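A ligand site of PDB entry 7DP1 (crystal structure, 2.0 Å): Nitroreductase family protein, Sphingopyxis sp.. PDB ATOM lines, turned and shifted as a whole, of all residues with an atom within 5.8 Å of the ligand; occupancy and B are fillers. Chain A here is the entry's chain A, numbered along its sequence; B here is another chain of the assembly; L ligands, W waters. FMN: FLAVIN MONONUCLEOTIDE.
An oxygen (O1P) of the ligand lies within hydrogen-bond range of the backbone NH (N) of Ser 20 (2.6 Å). The side-chain hydroxyl of Ser 20 lies within hydrogen-bond range of an oxygen (O3P) of the ligand, 2.8 Å away. The backbone NH (N) of Glu 176 sits at hydrogen-bond distance from a nitrogen (N5) of the ligand (2.8 Å). NH2 of Arg 219 is in salt-bridge range of O2P of the ligand (2.8 Å). N3 of the ligand is in hydrogen-bond range of OD1 of Asn 128. An oxygen (O2) of the ligand sits at hydrogen-bond distance from the guanidinium group (NE) of Arg 22 (2.8 Å). O3P of the ligand lies within salt-bridge range of NH1 of Arg 18 (3.0 Å). N of Cys 177 is in hydrogen-bond range of O4 of the ligand, 3.1 Å away. O4 of the ligand sits close to SG of Cys 177. The backbone NH (N) of Ser 46 of chain B is in hydrogen-bond range of an oxygen (O3') of the ligand (3.5 Å). The backbone carbonyl oxygen (O) of Ser 46 of chain B sits close to an oxygen (O3') of the ligand (3.4 Å).
A nitrogen (N10) of the ligand sits close to the backbone carbonyl oxygen (O) of Pro 174. Arg 19 touches the ligand. CG2 of Val 103 touches O4' of the ligand (3.4 Å). Phe 132 touches the ligand (CZ to O2, 3.9 Å). Gln 175 touches the ligand (CA to N5, 3.2 Å). CZ of Phe 198 touches C7M of the ligand, 3.7 Å away. Val 217 touches the ligand (CG1 to O5', 3.4 Å). CB of Pro 45 of chain B touches O3' of the ligand, 3.3 Å away. Gly 47 of chain B touches the ligand (N to C8M, 3.3 Å). Gly 48 of chain B touches the ligand. Asn 49 of chain B touches the ligand (CB to O4', 3.4 Å). Asp 153 of chain B touches the ligand. SD of Met 156 of chain B touches C8M of the ligand, 3.5 Å away. Hydrophobic or aromatic side chains within 4 Å of the ligand: Val 103, Phe 132, Pro 174, Phe 198, Val 217, Pro 45 of chain B and Met 156 of chain B. The nearest printed residue that does not touch the ligand is Cys 173 (4.1 Å).
Water W3 lies within hydrogen-bond range of O2P of the ligand (2.6 Å), NH2 of Arg 43 of chain B (2.9 Å) and O of Arg 18 (3.4 Å). Water W4 bridges an oxygen (O5') of the ligand (2.6 Å) and the guanidinium group of Arg 22 (3.2 Å). Water W2 bridges an oxygen (O2) of the ligand and the side-chain amide nitrogen (ND2) of Asn 128. Water W1 bridges O2' of the ligand (2.9 Å) and N of Gly 48 of chain B (3.0 Å).
SG of Cys 177 sits close to OD1 of Asn 128 (3.7 Å). The backbone carbonyl oxygen of Asn 128 lies within hydrogen-bond range of the side-chain amide nitrogen of Gln 175. The backbone carbonyl oxygen of Phe 125 is in hydrogen-bond range of the side-chain amide nitrogen of Asn 128, at 2.8 Å. O of Arg 43 of chain B lies within hydrogen-bond range of NH2 of Arg 18, at 3.0 Å. The side-chain amide nitrogen (NE2) of Gln 175 sits at hydrogen-bond distance from the side-chain sulfur (SG) of Cys 177, 3.5 Å away. The side-chain amide oxygen of Gln 175 sits at hydrogen-bond distance from the indole nitrogen of Trp 178, 2.9 Å away. The side-chain carboxylate of Asp 153 of chain B is in hydrogen-bond range of the backbone NH of Gly 47 of chain B (3.1 Å). The guanidinium group (NH2) of Arg 19 sits at hydrogen-bond distance from the backbone carbonyl oxygen (O) of Trp 215 (2.7 Å).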
ATOM      1  N   ARG A  18       8.851 -23.464 -20.741  1.00  0.00           N
ATOM      2  CA  ARG A  18       9.232 -23.163 -22.123  1.00  0.00           C
ATOM      3  C   ARG A  18      10.630 -22.567 -22.188  1.00  0.00           C
ATOM      4  O   ARG A  18      10.933 -21.600 -21.501  1.00  0.00           O
ATOM      5  CB  ARG A  18       8.235 -22.206 -22.791  1.00  0.00           C
ATOM      6  CG  ARG A  18       8.577 -21.936 -24.280  1.00  0.00           C
ATOM      7  CD  ARG A  18       8.427 -20.474 -24.718  1.00  0.00           C
ATOM      8  NE  ARG A  18       9.216 -19.574 -23.869  1.00  0.00           N
ATOM      9  CZ  ARG A  18      10.505 -19.326 -24.011  1.00  0.00           C
ATOM     10  NH1 ARG A  18      11.190 -19.937 -24.973  1.00  0.00           N
ATOM     11  NH2 ARG A  18      11.126 -18.492 -23.163  1.00  0.00           N
ATOM     12  N   ARG A  19      11.498 -23.159 -23.010  1.00  0.00           N
ATOM     13  CA  ARG A  19      12.803 -22.563 -23.255  1.00  0.00           C
ATOM     14  C   ARG A  19      13.167 -22.686 -24.726  1.00  0.00           C
ATOM     15  O   ARG A  19      12.562 -23.453 -25.475  1.00  0.00           O
ATOM     16  CB  ARG A  19      13.875 -23.211 -22.382  1.00  0.00           C
ATOM     17  CG  ARG A  19      14.259 -24.630 -22.764  1.00  0.00           C
ATOM     18  CD  ARG A  19      15.328 -25.185 -21.795  1.00  0.00           C
ATOM     19  NE  ARG A  19      16.594 -24.456 -21.892  1.00  0.00           N
ATOM     20  CZ  ARG A  19      17.428 -24.195 -20.888  1.00  0.00           C
ATOM     21  NH1 ARG A  19      17.186 -24.634 -19.654  1.00  0.00           N
ATOM     22  NH2 ARG A  19      18.538 -23.509 -21.125  1.00  0.00           N
ATOM     23  N   SER A  20      14.159 -21.920 -25.157  1.00  0.00           N
ATOM     24  CA  SER A  20      14.636 -22.069 -26.507  1.00  0.00           C
ATOM     25  C   SER A  20      15.506 -23.327 -26.577  1.00  0.00           C
ATOM     26  O   SER A  20      16.667 -23.292 -26.202  1.00  0.00           O
ATOM     27  CB  SER A  20      15.388 -20.818 -26.947  1.00  0.00           C
ATOM     28  OG  SER A  20      14.467 -19.736 -27.066  1.00  0.00           O
ATOM     29  N   VAL A  21      14.943 -24.412 -27.094  1.00  0.00           N
ATOM     30  CA  VAL A  21      15.626 -25.702 -27.137  1.00  0.00           C
ATOM     31  C   VAL A  21      16.553 -25.827 -28.356  1.00  0.00           C
ATOM     32  O   VAL A  21      16.132 -25.640 -29.497  1.00  0.00           O
ATOM     33  CB  VAL A  21      14.584 -26.845 -27.150  1.00  0.00           C
ATOM     34  CG1 VAL A  21      15.211 -28.161 -27.507  1.00  0.00           C
ATOM     35  CG2 VAL A  21      13.896 -26.914 -25.790  1.00  0.00           C
ATOM     36  N   ARG A  22      17.812 -26.159 -28.103  1.00  0.00           N
ATOM     37  CA  ARG A  22      18.795 -26.241 -29.189  1.00  0.00           C
ATOM     38  C   ARG A  22      19.399 -27.641 -29.291  1.00  0.00           C
ATOM     39  O   ARG A  22      20.560 -27.803 -29.684  1.00  0.00           O
ATOM     40  CB  ARG A  22      19.882 -25.178 -29.008  1.00  0.00           C
ATOM     41  CG  ARG A  22      19.294 -23.770 -29.011  1.00  0.00           C
ATOM     42  CD  ARG A  22      20.286 -22.669 -28.694  1.00  0.00           C
ATOM     43  NE  ARG A  22      19.630 -21.357 -28.719  1.00  0.00           N
ATOM     44  CZ  ARG A  22      19.237 -20.685 -27.650  1.00  0.00           C
ATOM     45  NH1 ARG A  22      19.440 -21.195 -26.439  1.00  0.00           N
ATOM     46  NH2 ARG A  22      18.638 -19.502 -27.767  1.00  0.00           N
ATOM     47  N   VAL A 103      23.381 -14.247 -22.102  1.00  0.00           N
ATOM     48  CA  VAL A 103      22.722 -15.504 -22.391  1.00  0.00           C
ATOM     49  C   VAL A 103      23.646 -16.256 -23.334  1.00  0.00           C
ATOM     50  O   VAL A 103      23.656 -17.490 -23.392  1.00  0.00           O
ATOM     51  CB  VAL A 103      21.309 -15.331 -23.000  1.00  0.00           C
ATOM     52  CG1 VAL A 103      21.369 -14.654 -24.365  1.00  0.00           C
ATOM     53  CG2 VAL A 103      20.610 -16.663 -23.111  1.00  0.00           C
ATOM     54  N   LEU A 107      24.862 -20.230 -22.846  1.00  0.00           N
ATOM     55  CA  LEU A 107      24.606 -21.145 -23.965  1.00  0.00           C
ATOM     56  C   LEU A 107      25.849 -21.919 -24.396  1.00  0.00           C
ATOM     57  O   LEU A 107      25.784 -23.117 -24.649  1.00  0.00           O
ATOM     58  CB  LEU A 107      24.047 -20.376 -25.159  1.00  0.00           C
ATOM     59  CG  LEU A 107      23.927 -21.130 -26.493  1.00  0.00           C
ATOM     60  CD1 LEU A 107      23.110 -22.399 -26.323  1.00  0.00           C
ATOM     61  CD2 LEU A 107      23.309 -20.251 -27.582  1.00  0.00           C
ATOM     62  N   PHE A 125      27.075 -22.190 -33.834  1.00  0.00           N
ATOM     63  CA  PHE A 125      26.058 -21.241 -34.310  1.00  0.00           C
ATOM     64  C   PHE A 125      25.438 -21.662 -35.643  1.00  0.00           C
ATOM     65  O   PHE A 125      24.259 -21.447 -35.879  1.00  0.00           O
ATOM     66  CB  PHE A 125      26.646 -19.837 -34.474  1.00  0.00           C
ATOM     67  CG  PHE A 125      25.666 -18.821 -35.014  1.00  0.00           C
ATOM     68  CD1 PHE A 125      25.668 -18.490 -36.368  1.00  0.00           C
ATOM     69  CD2 PHE A 125      24.723 -18.241 -34.196  1.00  0.00           C
ATOM     70  CE1 PHE A 125      24.755 -17.579 -36.885  1.00  0.00           C
ATOM     71  CE2 PHE A 125      23.810 -17.310 -34.701  1.00  0.00           C
ATOM     72  CZ  PHE A 125      23.828 -16.993 -36.049  1.00  0.00           C
ATOM     73  N   ASN A 128      22.147 -23.557 -36.176  1.00  0.00           N
ATOM     74  CA  ASN A 128      20.884 -22.825 -36.322  1.00  0.00           C
ATOM     75  C   ASN A 128      20.237 -23.184 -37.655  1.00  0.00           C
ATOM     76  O   ASN A 128      19.013 -23.336 -37.759  1.00  0.00           O
ATOM     77  CB  ASN A 128      21.112 -21.309 -36.273  1.00  0.00           C
ATOM     78  CG  ASN A 128      21.018 -20.722 -34.865  1.00  0.00           C
ATOM     79  OD1 ASN A 128      19.949 -20.318 -34.432  1.00  0.00           O
ATOM     80  ND2 ASN A 128      22.157 -20.628 -34.186  1.00  0.00           N
ATOM     81  N   PHE A 132      18.770 -26.910 -35.350  1.00  0.00           N
ATOM     82  CA  PHE A 132      19.332 -27.659 -34.230  1.00  0.00           C
ATOM     83  C   PHE A 132      18.855 -29.094 -34.245  1.00  0.00           C
ATOM     84  O   PHE A 132      18.706 -29.714 -33.197  1.00  0.00           O
ATOM     85  CB  PHE A 132      18.959 -27.002 -32.886  1.00  0.00           C
ATOM     86  CG  PHE A 132      19.428 -25.585 -32.748  1.00  0.00           C
ATOM     87  CD1 PHE A 132      20.778 -25.283 -32.765  1.00  0.00           C
ATOM     88  CD2 PHE A 132      18.515 -24.550 -32.618  1.00  0.00           C
ATOM     89  CE1 PHE A 132      21.208 -23.975 -32.632  1.00  0.00           C
ATOM     90  CE2 PHE A 132      18.950 -23.237 -32.501  1.00  0.00           C
ATOM     91  CZ  PHE A 132      20.298 -22.954 -32.506  1.00  0.00           C
ATOM     92  N   LEU A 158       2.836 -16.304 -31.961  1.00  0.00           N
ATOM     93  CA  LEU A 158       3.984 -17.176 -31.812  1.00  0.00           C
ATOM     94  C   LEU A 158       4.149 -17.693 -30.396  1.00  0.00           C
ATOM     95  O   LEU A 158       4.412 -18.871 -30.179  1.00  0.00           O
ATOM     96  CB  LEU A 158       5.278 -16.445 -32.243  1.00  0.00           C
ATOM     97  CG  LEU A 158       6.446 -17.407 -32.365  1.00  0.00           C
ATOM     98  CD1 LEU A 158       6.188 -18.434 -33.481  1.00  0.00           C
ATOM     99  CD2 LEU A 158       7.751 -16.661 -32.589  1.00  0.00           C
ATOM    100  N   MET A 162       4.259 -21.566 -28.948  1.00  0.00           N
ATOM    101  CA  MET A 162       5.361 -22.100 -28.157  1.00  0.00           C
ATOM    102  C   MET A 162       4.869 -22.654 -26.817  1.00  0.00           C
ATOM    103  O   MET A 162       5.331 -23.685 -26.342  1.00  0.00           O
ATOM    104  CB  MET A 162       6.390 -21.000 -27.955  1.00  0.00           C
ATOM    105  CG  MET A 162       7.133 -20.642 -29.251  1.00  0.00           C
ATOM    106  SD  MET A 162       8.475 -19.510 -28.902  1.00  0.00           S
ATOM    107  CE  MET A 162       7.581 -17.979 -28.817  1.00  0.00           C
ATOM    108  N   CYS A 173      12.369 -23.749 -30.779  1.00  0.00           N
ATOM    109  CA  CYS A 173      13.343 -22.671 -30.760  1.00  0.00           C
ATOM    110  C   CYS A 173      12.906 -21.633 -31.766  1.00  0.00           C
ATOM    111  O   CYS A 173      12.921 -21.889 -32.958  1.00  0.00           O
ATOM    112  CB  CYS A 173      14.749 -23.190 -31.121  1.00  0.00           C
ATOM    113  SG  CYS A 173      16.038 -21.947 -30.777  1.00  0.00           S
ATOM    114  N   PRO A 174      12.481 -20.443 -31.295  1.00  0.00           N
ATOM    115  CA  PRO A 174      12.251 -19.356 -32.234  1.00  0.00           C
ATOM    116  C   PRO A 174      13.589 -18.961 -32.860  1.00  0.00           C
ATOM    117  O   PRO A 174      14.599 -18.981 -32.168  1.00  0.00           O
ATOM    118  CB  PRO A 174      11.663 -18.244 -31.369  1.00  0.00           C
ATOM    119  CG  PRO A 174      12.126 -18.568 -29.985  1.00  0.00           C
ATOM    120  CD  PRO A 174      12.248 -20.036 -29.891  1.00  0.00           C
ATOM    121  N   GLN A 175      13.611 -18.671 -34.153  1.00  0.00           N
ATOM    122  CA  GLN A 175      14.882 -18.402 -34.853  1.00  0.00           C
ATOM    123  C   GLN A 175      14.794 -17.249 -35.834  1.00  0.00           C
ATOM    124  O   GLN A 175      14.215 -17.405 -36.901  1.00  0.00           O
ATOM    125  CB  GLN A 175      15.355 -19.624 -35.625  1.00  0.00           C
ATOM    126  CG  GLN A 175      15.777 -20.809 -34.810  1.00  0.00           C
ATOM    127  CD  GLN A 175      16.413 -21.853 -35.704  1.00  0.00           C
ATOM    128  OE1 GLN A 175      15.716 -22.588 -36.411  1.00  0.00           O
ATOM    129  NE2 GLN A 175      17.744 -21.915 -35.705  1.00  0.00           N
ATOM    130  N   GLU A 176      15.422 -16.125 -35.512  1.00  0.00           N
ATOM    131  CA  GLU A 176      15.469 -15.006 -36.443  1.00  0.00           C
ATOM    132  C   GLU A 176      16.597 -15.178 -37.456  1.00  0.00           C
ATOM    133  O   GLU A 176      16.706 -14.405 -38.407  1.00  0.00           O
ATOM    134  CB  GLU A 176      15.648 -13.698 -35.698  1.00  0.00           C
ATOM    135  CG  GLU A 176      14.383 -12.921 -35.558  1.00  0.00           C
ATOM    136  CD  GLU A 176      14.412 -12.018 -34.346  1.00  0.00           C
ATOM    137  OE1 GLU A 176      15.470 -11.901 -33.693  1.00  0.00           O
ATOM    138  OE2 GLU A 176      13.348 -11.424 -34.041  1.00  0.00           O
ATOM    139  N   CYS A 177      17.444 -16.167 -37.228  1.00  0.00           N
ATOM    140  CA  CYS A 177      18.605 -16.363 -38.097  1.00  0.00           C
ATOM    141  C   CYS A 177      18.204 -16.554 -39.570  1.00  0.00           C
ATOM    142  O   CYS A 177      18.941 -16.183 -40.485  1.00  0.00           O
ATOM    143  CB  CYS A 177      19.428 -17.567 -37.624  1.00  0.00           C
ATOM    144  SG  CYS A 177      18.486 -19.112 -37.588  1.00  0.00           S
ATOM    145  N   TRP A 178      17.015 -17.114 -39.794  1.00  0.00           N
ATOM    146  CA  TRP A 178      16.513 -17.358 -41.154  1.00  0.00           C
ATOM    147  C   TRP A 178      16.244 -16.052 -41.906  1.00  0.00           C
ATOM    148  O   TRP A 178      16.308 -16.008 -43.138  1.00  0.00           O
ATOM    149  CB  TRP A 178      15.240 -18.222 -41.087  1.00  0.00           C
ATOM    150  CG  TRP A 178      15.527 -19.589 -40.492  1.00  0.00           C
ATOM    151  CD1 TRP A 178      15.258 -20.005 -39.221  1.00  0.00           C
ATOM    152  CD2 TRP A 178      16.203 -20.681 -41.142  1.00  0.00           C
ATOM    153  NE1 TRP A 178      15.712 -21.290 -39.036  1.00  0.00           N
ATOM    154  CE2 TRP A 178      16.294 -21.733 -40.204  1.00  0.00           C
ATOM    155  CE3 TRP A 178      16.726 -20.883 -42.427  1.00  0.00           C
ATOM    156  CZ2 TRP A 178      16.883 -22.959 -40.507  1.00  0.00           C
ATOM    157  CZ3 TRP A 178      17.325 -22.106 -42.732  1.00  0.00           C
ATOM    158  CH2 TRP A 178      17.390 -23.123 -41.778  1.00  0.00           C
ATOM    159  N   PHE A 198       9.470 -13.075 -41.079  1.00  0.00           N
ATOM    160  CA  PHE A 198       9.849 -12.601 -39.744  1.00  0.00           C
ATOM    161  C   PHE A 198      10.832 -13.577 -39.098  1.00  0.00           C
ATOM    162  O   PHE A 198      11.975 -13.225 -38.787  1.00  0.00           O
ATOM    163  CB  PHE A 198       8.596 -12.379 -38.867  1.00  0.00           C
ATOM    164  CG  PHE A 198       8.871 -12.329 -37.363  1.00  0.00           C
ATOM    165  CD1 PHE A 198       9.991 -11.715 -36.849  1.00  0.00           C
ATOM    166  CD2 PHE A 198       7.967 -12.879 -36.472  1.00  0.00           C
ATOM    167  CE1 PHE A 198      10.212 -11.670 -35.479  1.00  0.00           C
ATOM    168  CE2 PHE A 198       8.173 -12.834 -35.112  1.00  0.00           C
ATOM    169  CZ  PHE A 198       9.313 -12.234 -34.616  1.00  0.00           C
ATOM    170  N   SER A 199      10.415 -14.809 -38.907  1.00  0.00           N
ATOM    171  CA  SER A 199      11.228 -15.697 -38.086  1.00  0.00           C
ATOM    172  C   SER A 199      10.938 -17.149 -38.400  1.00  0.00           C
ATOM    173  O   SER A 199       9.871 -17.478 -38.920  1.00  0.00           O
ATOM    174  CB  SER A 199      10.965 -15.410 -36.608  1.00  0.00           C
ATOM    175  OG  SER A 199      11.695 -16.307 -35.780  1.00  0.00           O
ATOM    176  N   TRP A 215      20.830 -25.531 -18.694  1.00  0.00           N
ATOM    177  CA  TRP A 215      21.319 -24.369 -17.950  1.00  0.00           C
ATOM    178  C   TRP A 215      20.191 -23.382 -17.692  1.00  0.00           C
ATOM    179  O   TRP A 215      19.303 -23.210 -18.518  1.00  0.00           O
ATOM    180  CB  TRP A 215      22.475 -23.703 -18.716  1.00  0.00           C
ATOM    181  CG  TRP A 215      22.112 -23.334 -20.122  1.00  0.00           C
ATOM    182  CD1 TRP A 215      22.161 -24.148 -21.224  1.00  0.00           C
ATOM    183  CD2 TRP A 215      21.615 -22.075 -20.587  1.00  0.00           C
ATOM    184  NE1 TRP A 215      21.748 -23.468 -22.346  1.00  0.00           N
ATOM    185  CE2 TRP A 215      21.396 -22.195 -21.980  1.00  0.00           C
ATOM    186  CE3 TRP A 215      21.330 -20.855 -19.965  1.00  0.00           C
ATOM    187  CZ2 TRP A 215      20.913 -21.141 -22.758  1.00  0.00           C
ATOM    188  CZ3 TRP A 215      20.861 -19.801 -20.733  1.00  0.00           C
ATOM    189  CH2 TRP A 215      20.652 -19.951 -22.119  1.00  0.00           C
ATOM    190  N   VAL A 217      18.196 -20.069 -17.550  1.00  0.00           N
ATOM    191  CA  VAL A 217      18.214 -18.913 -18.440  1.00  0.00           C
ATOM    192  C   VAL A 217      17.845 -17.641 -17.706  1.00  0.00           C
ATOM    193  O   VAL A 217      16.722 -17.517 -17.197  1.00  0.00           O
ATOM    194  CB  VAL A 217      17.252 -19.109 -19.614  1.00  0.00           C
ATOM    195  CG1 VAL A 217      17.456 -18.012 -20.641  1.00  0.00           C
ATOM    196  CG2 VAL A 217      17.464 -20.493 -20.224  1.00  0.00           C
ATOM    197  N   ARG A 219      16.925 -13.717 -16.541  1.00  0.00           N
ATOM    198  CA  ARG A 219      16.063 -12.611 -16.918  1.00  0.00           C
ATOM    199  C   ARG A 219      16.394 -11.460 -16.006  1.00  0.00           C
ATOM    200  O   ARG A 219      16.887 -11.670 -14.897  1.00  0.00           O
ATOM    201  CB  ARG A 219      14.581 -12.971 -16.791  1.00  0.00           C
ATOM    202  CG  ARG A 219      14.033 -13.976 -17.814  1.00  0.00           C
ATOM    203  CD  ARG A 219      14.022 -13.388 -19.231  1.00  0.00           C
ATOM    204  NE  ARG A 219      13.313 -14.269 -20.153  1.00  0.00           N
ATOM    205  CZ  ARG A 219      13.810 -15.388 -20.647  1.00  0.00           C
ATOM    206  NH1 ARG A 219      15.029 -15.786 -20.306  1.00  0.00           N
ATOM    207  NH2 ARG A 219      13.074 -16.123 -21.470  1.00  0.00           N
ATOM    208  N   ARG B  43       9.347 -14.536 -18.222  1.00  0.00           N
ATOM    209  CA  ARG B  43       9.923 -15.743 -18.839  1.00  0.00           C
ATOM    210  C   ARG B  43       9.583 -15.847 -20.320  1.00  0.00           C
ATOM    211  O   ARG B  43       9.946 -16.823 -20.973  1.00  0.00           O
ATOM    212  CB  ARG B  43       9.492 -17.001 -18.094  1.00  0.00           C
ATOM    213  CG  ARG B  43       9.871 -17.039 -16.608  1.00  0.00           C
ATOM    214  CD  ARG B  43      11.374 -16.814 -16.391  1.00  0.00           C
ATOM    215  NE  ARG B  43      12.211 -17.772 -17.108  1.00  0.00           N
ATOM    216  CZ  ARG B  43      13.529 -17.836 -17.020  1.00  0.00           C
ATOM    217  NH1 ARG B  43      14.181 -16.971 -16.247  1.00  0.00           N
ATOM    218  NH2 ARG B  43      14.203 -18.732 -17.716  1.00  0.00           N
ATOM    219  N   ALA B  44       8.872 -14.852 -20.853  1.00  0.00           N
ATOM    220  CA  ALA B  44       8.635 -14.794 -22.289  1.00  0.00           C
ATOM    221  C   ALA B  44       9.970 -14.714 -23.042  1.00  0.00           C
ATOM    222  O   ALA B  44      10.915 -14.074 -22.578  1.00  0.00           O
ATOM    223  CB  ALA B  44       7.760 -13.569 -22.646  1.00  0.00           C
ATOM    224  N   PRO B  45      10.052 -15.332 -24.219  1.00  0.00           N
ATOM    225  CA  PRO B  45      11.335 -15.251 -24.929  1.00  0.00           C
ATOM    226  C   PRO B  45      11.498 -13.922 -25.643  1.00  0.00           C
ATOM    227  O   PRO B  45      10.545 -13.160 -25.749  1.00  0.00           O
ATOM    228  CB  PRO B  45      11.236 -16.385 -25.949  1.00  0.00           C
ATOM    229  CG  PRO B  45       9.738 -16.376 -26.324  1.00  0.00           C
ATOM    230  CD  PRO B  45       9.007 -15.985 -25.024  1.00  0.00           C
ATOM    231  N   SER B  46      12.693 -13.638 -26.134  1.00  0.00           N
ATOM    232  CA  SER B  46      12.891 -12.455 -26.951  1.00  0.00           C
ATOM    233  C   SER B  46      14.140 -12.677 -27.742  1.00  0.00           C
ATOM    234  O   SER B  46      15.044 -13.370 -27.274  1.00  0.00           O
ATOM    235  CB  SER B  46      13.009 -11.173 -26.118  1.00  0.00           C
ATOM    236  OG  SER B  46      14.118 -11.215 -25.245  1.00  0.00           O
ATOM    237  N   GLY B  47      14.185 -12.110 -28.946  1.00  0.00           N
ATOM    238  CA  GLY B  47      15.377 -12.238 -29.767  1.00  0.00           C
ATOM    239  C   GLY B  47      16.562 -11.783 -28.961  1.00  0.00           C
ATOM    240  O   GLY B  47      16.535 -10.698 -28.386  1.00  0.00           O
ATOM    241  N   GLY B  48      17.573 -12.633 -28.879  1.00  0.00           N
ATOM    242  CA  GLY B  48      18.805 -12.297 -28.183  1.00  0.00           C
ATOM    243  C   GLY B  48      18.582 -12.077 -26.702  1.00  0.00           C
ATOM    244  O   GLY B  48      19.447 -11.520 -26.023  1.00  0.00           O
ATOM    245  N   ASN B  49      17.435 -12.514 -26.188  1.00  0.00           N
ATOM    246  CA  ASN B  49      17.079 -12.211 -24.779  1.00  0.00           C
ATOM    247  C   ASN B  49      17.163 -10.715 -24.462  1.00  0.00           C
ATOM    248  O   ASN B  49      17.502 -10.326 -23.343  1.00  0.00           O
ATOM    249  CB  ASN B  49      17.979 -12.995 -23.811  1.00  0.00           C
ATOM    250  CG  ASN B  49      17.360 -13.150 -22.440  1.00  0.00           C
ATOM    251  OD1 ASN B  49      16.152 -13.339 -22.303  1.00  0.00           O
ATOM    252  ND2 ASN B  49      18.201 -13.105 -21.425  1.00  0.00           N
ATOM    253  N   PRO B 149      11.220  -6.701 -35.107  1.00  0.00           N
ATOM    254  CA  PRO B 149      11.267  -7.933 -34.309  1.00  0.00           C
ATOM    255  C   PRO B 149      11.150  -7.684 -32.779  1.00  0.00           C
ATOM    256  O   PRO B 149      10.583  -8.519 -32.079  1.00  0.00           O
ATOM    257  CB  PRO B 149      12.621  -8.530 -34.658  1.00  0.00           C
ATOM    258  CG  PRO B 149      13.473  -7.316 -35.028  1.00  0.00           C
ATOM    259  CD  PRO B 149      12.509  -6.434 -35.784  1.00  0.00           C
ATOM    260  N   ALA B 152       7.759  -7.526 -31.944  1.00  0.00           N
ATOM    261  CA  ALA B 152       7.198  -8.870 -31.849  1.00  0.00           C
ATOM    262  C   ALA B 152       7.488  -9.472 -30.481  1.00  0.00           C
ATOM    263  O   ALA B 152       6.616 -10.134 -29.908  1.00  0.00           O
ATOM    264  CB  ALA B 152       7.709  -9.793 -32.988  1.00  0.00           C
ATOM    265  N   ASP B 153       8.691  -9.238 -29.955  1.00  0.00           N
ATOM    266  CA  ASP B 153       9.028  -9.652 -28.562  1.00  0.00           C
ATOM    267  C   ASP B 153       8.037  -9.068 -27.532  1.00  0.00           C
ATOM    268  O   ASP B 153       7.640  -9.736 -26.582  1.00  0.00           O
ATOM    269  CB  ASP B 153      10.424  -9.174 -28.110  1.00  0.00           C
ATOM    270  CG  ASP B 153      11.589  -9.703 -28.973  1.00  0.00           C
ATOM    271  OD1 ASP B 153      12.648  -9.039 -28.956  1.00  0.00           O
ATOM    272  OD2 ASP B 153      11.464 -10.753 -29.644  1.00  0.00           O
ATOM    273  N   MET B 156       4.962 -11.063 -27.499  1.00  0.00           N
ATOM    274  CA  MET B 156       5.148 -12.309 -26.750  1.00  0.00           C
ATOM    275  C   MET B 156       4.927 -12.116 -25.252  1.00  0.00           C
ATOM    276  O   MET B 156       4.230 -12.887 -24.597  1.00  0.00           O
ATOM    277  CB  MET B 156       6.550 -12.866 -27.025  1.00  0.00           C
ATOM    278  CG  MET B 156       6.700 -13.331 -28.462  1.00  0.00           C
ATOM    279  SD  MET B 156       8.400 -13.793 -28.872  1.00  0.00           S
ATOM    280  CE  MET B 156       8.367 -13.582 -30.650  1.00  0.00           C
HETATM  281  N1  FMN L   1      17.916 -18.297 -30.494  1.00  0.00           N
HETATM  282  C2  FMN L   1      18.916 -18.764 -31.312  1.00  0.00           C
HETATM  283  O2  FMN L   1      19.790 -19.500 -30.871  1.00  0.00           O
HETATM  284  N3  FMN L   1      18.961 -18.396 -32.638  1.00  0.00           N
HETATM  285  C4  FMN L   1      18.008 -17.567 -33.177  1.00  0.00           C
HETATM  286  O4  FMN L   1      18.060 -17.273 -34.381  1.00  0.00           O
HETATM  287  C4A FMN L   1      16.993 -17.095 -32.337  1.00  0.00           C
HETATM  288  N5  FMN L   1      16.019 -16.246 -32.826  1.00  0.00           N
HETATM  289  C5A FMN L   1      15.009 -15.787 -32.013  1.00  0.00           C
HETATM  290  C6  FMN L   1      14.039 -14.951 -32.567  1.00  0.00           C
HETATM  291  C7  FMN L   1      13.008 -14.471 -31.765  1.00  0.00           C
HETATM  292  C7M FMN L   1      11.954 -13.580 -32.331  1.00  0.00           C
HETATM  293  C8  FMN L   1      12.952 -14.828 -30.433  1.00  0.00           C
HETATM  294  C8M FMN L   1      11.799 -14.289 -29.627  1.00  0.00           C
HETATM  295  C9  FMN L   1      13.924 -15.659 -29.871  1.00  0.00           C
HETATM  296  C9A FMN L   1      14.958 -16.147 -30.668  1.00  0.00           C
HETATM  297  N10 FMN L   1      15.952 -16.980 -30.168  1.00  0.00           N
HETATM  298  C10 FMN L   1      16.961 -17.444 -30.990  1.00  0.00           C
HETATM  299  C1' FMN L   1      15.940 -17.421 -28.738  1.00  0.00           C
HETATM  300  C2' FMN L   1      16.410 -16.382 -27.725  1.00  0.00           C
HETATM  301  O2' FMN L   1      17.814 -16.343 -27.720  1.00  0.00           O
HETATM  302  C3' FMN L   1      15.904 -16.799 -26.354  1.00  0.00           C
HETATM  303  O3' FMN L   1      14.512 -16.592 -26.357  1.00  0.00           O
HETATM  304  C4' FMN L   1      16.492 -15.983 -25.198  1.00  0.00           C
HETATM  305  O4' FMN L   1      17.879 -16.167 -25.028  1.00  0.00           O
HETATM  306  C5' FMN L   1      15.810 -16.442 -23.929  1.00  0.00           C
HETATM  307  O5' FMN L   1      16.104 -17.815 -23.768  1.00  0.00           O
HETATM  308  P   FMN L   1      14.853 -18.792 -23.531  1.00  0.00           P
HETATM  309  O1P FMN L   1      15.331 -20.214 -23.635  1.00  0.00           O
HETATM  310  O2P FMN L   1      14.250 -18.515 -22.163  1.00  0.00           O
HETATM  311  O3P FMN L   1      13.803 -18.508 -24.589  1.00  0.00           O
HETATM  312  O   HOH W   1      18.916 -15.060 -30.073  1.00  0.00           O
HETATM  313  O   HOH W   2      22.383 -19.118 -31.590  1.00  0.00           O
HETATM  314  O   HOH W   3      13.706 -20.065 -20.205  1.00  0.00           O
HETATM  315  O   HOH W   4      18.349 -18.891 -24.557  1.00  0.00           O
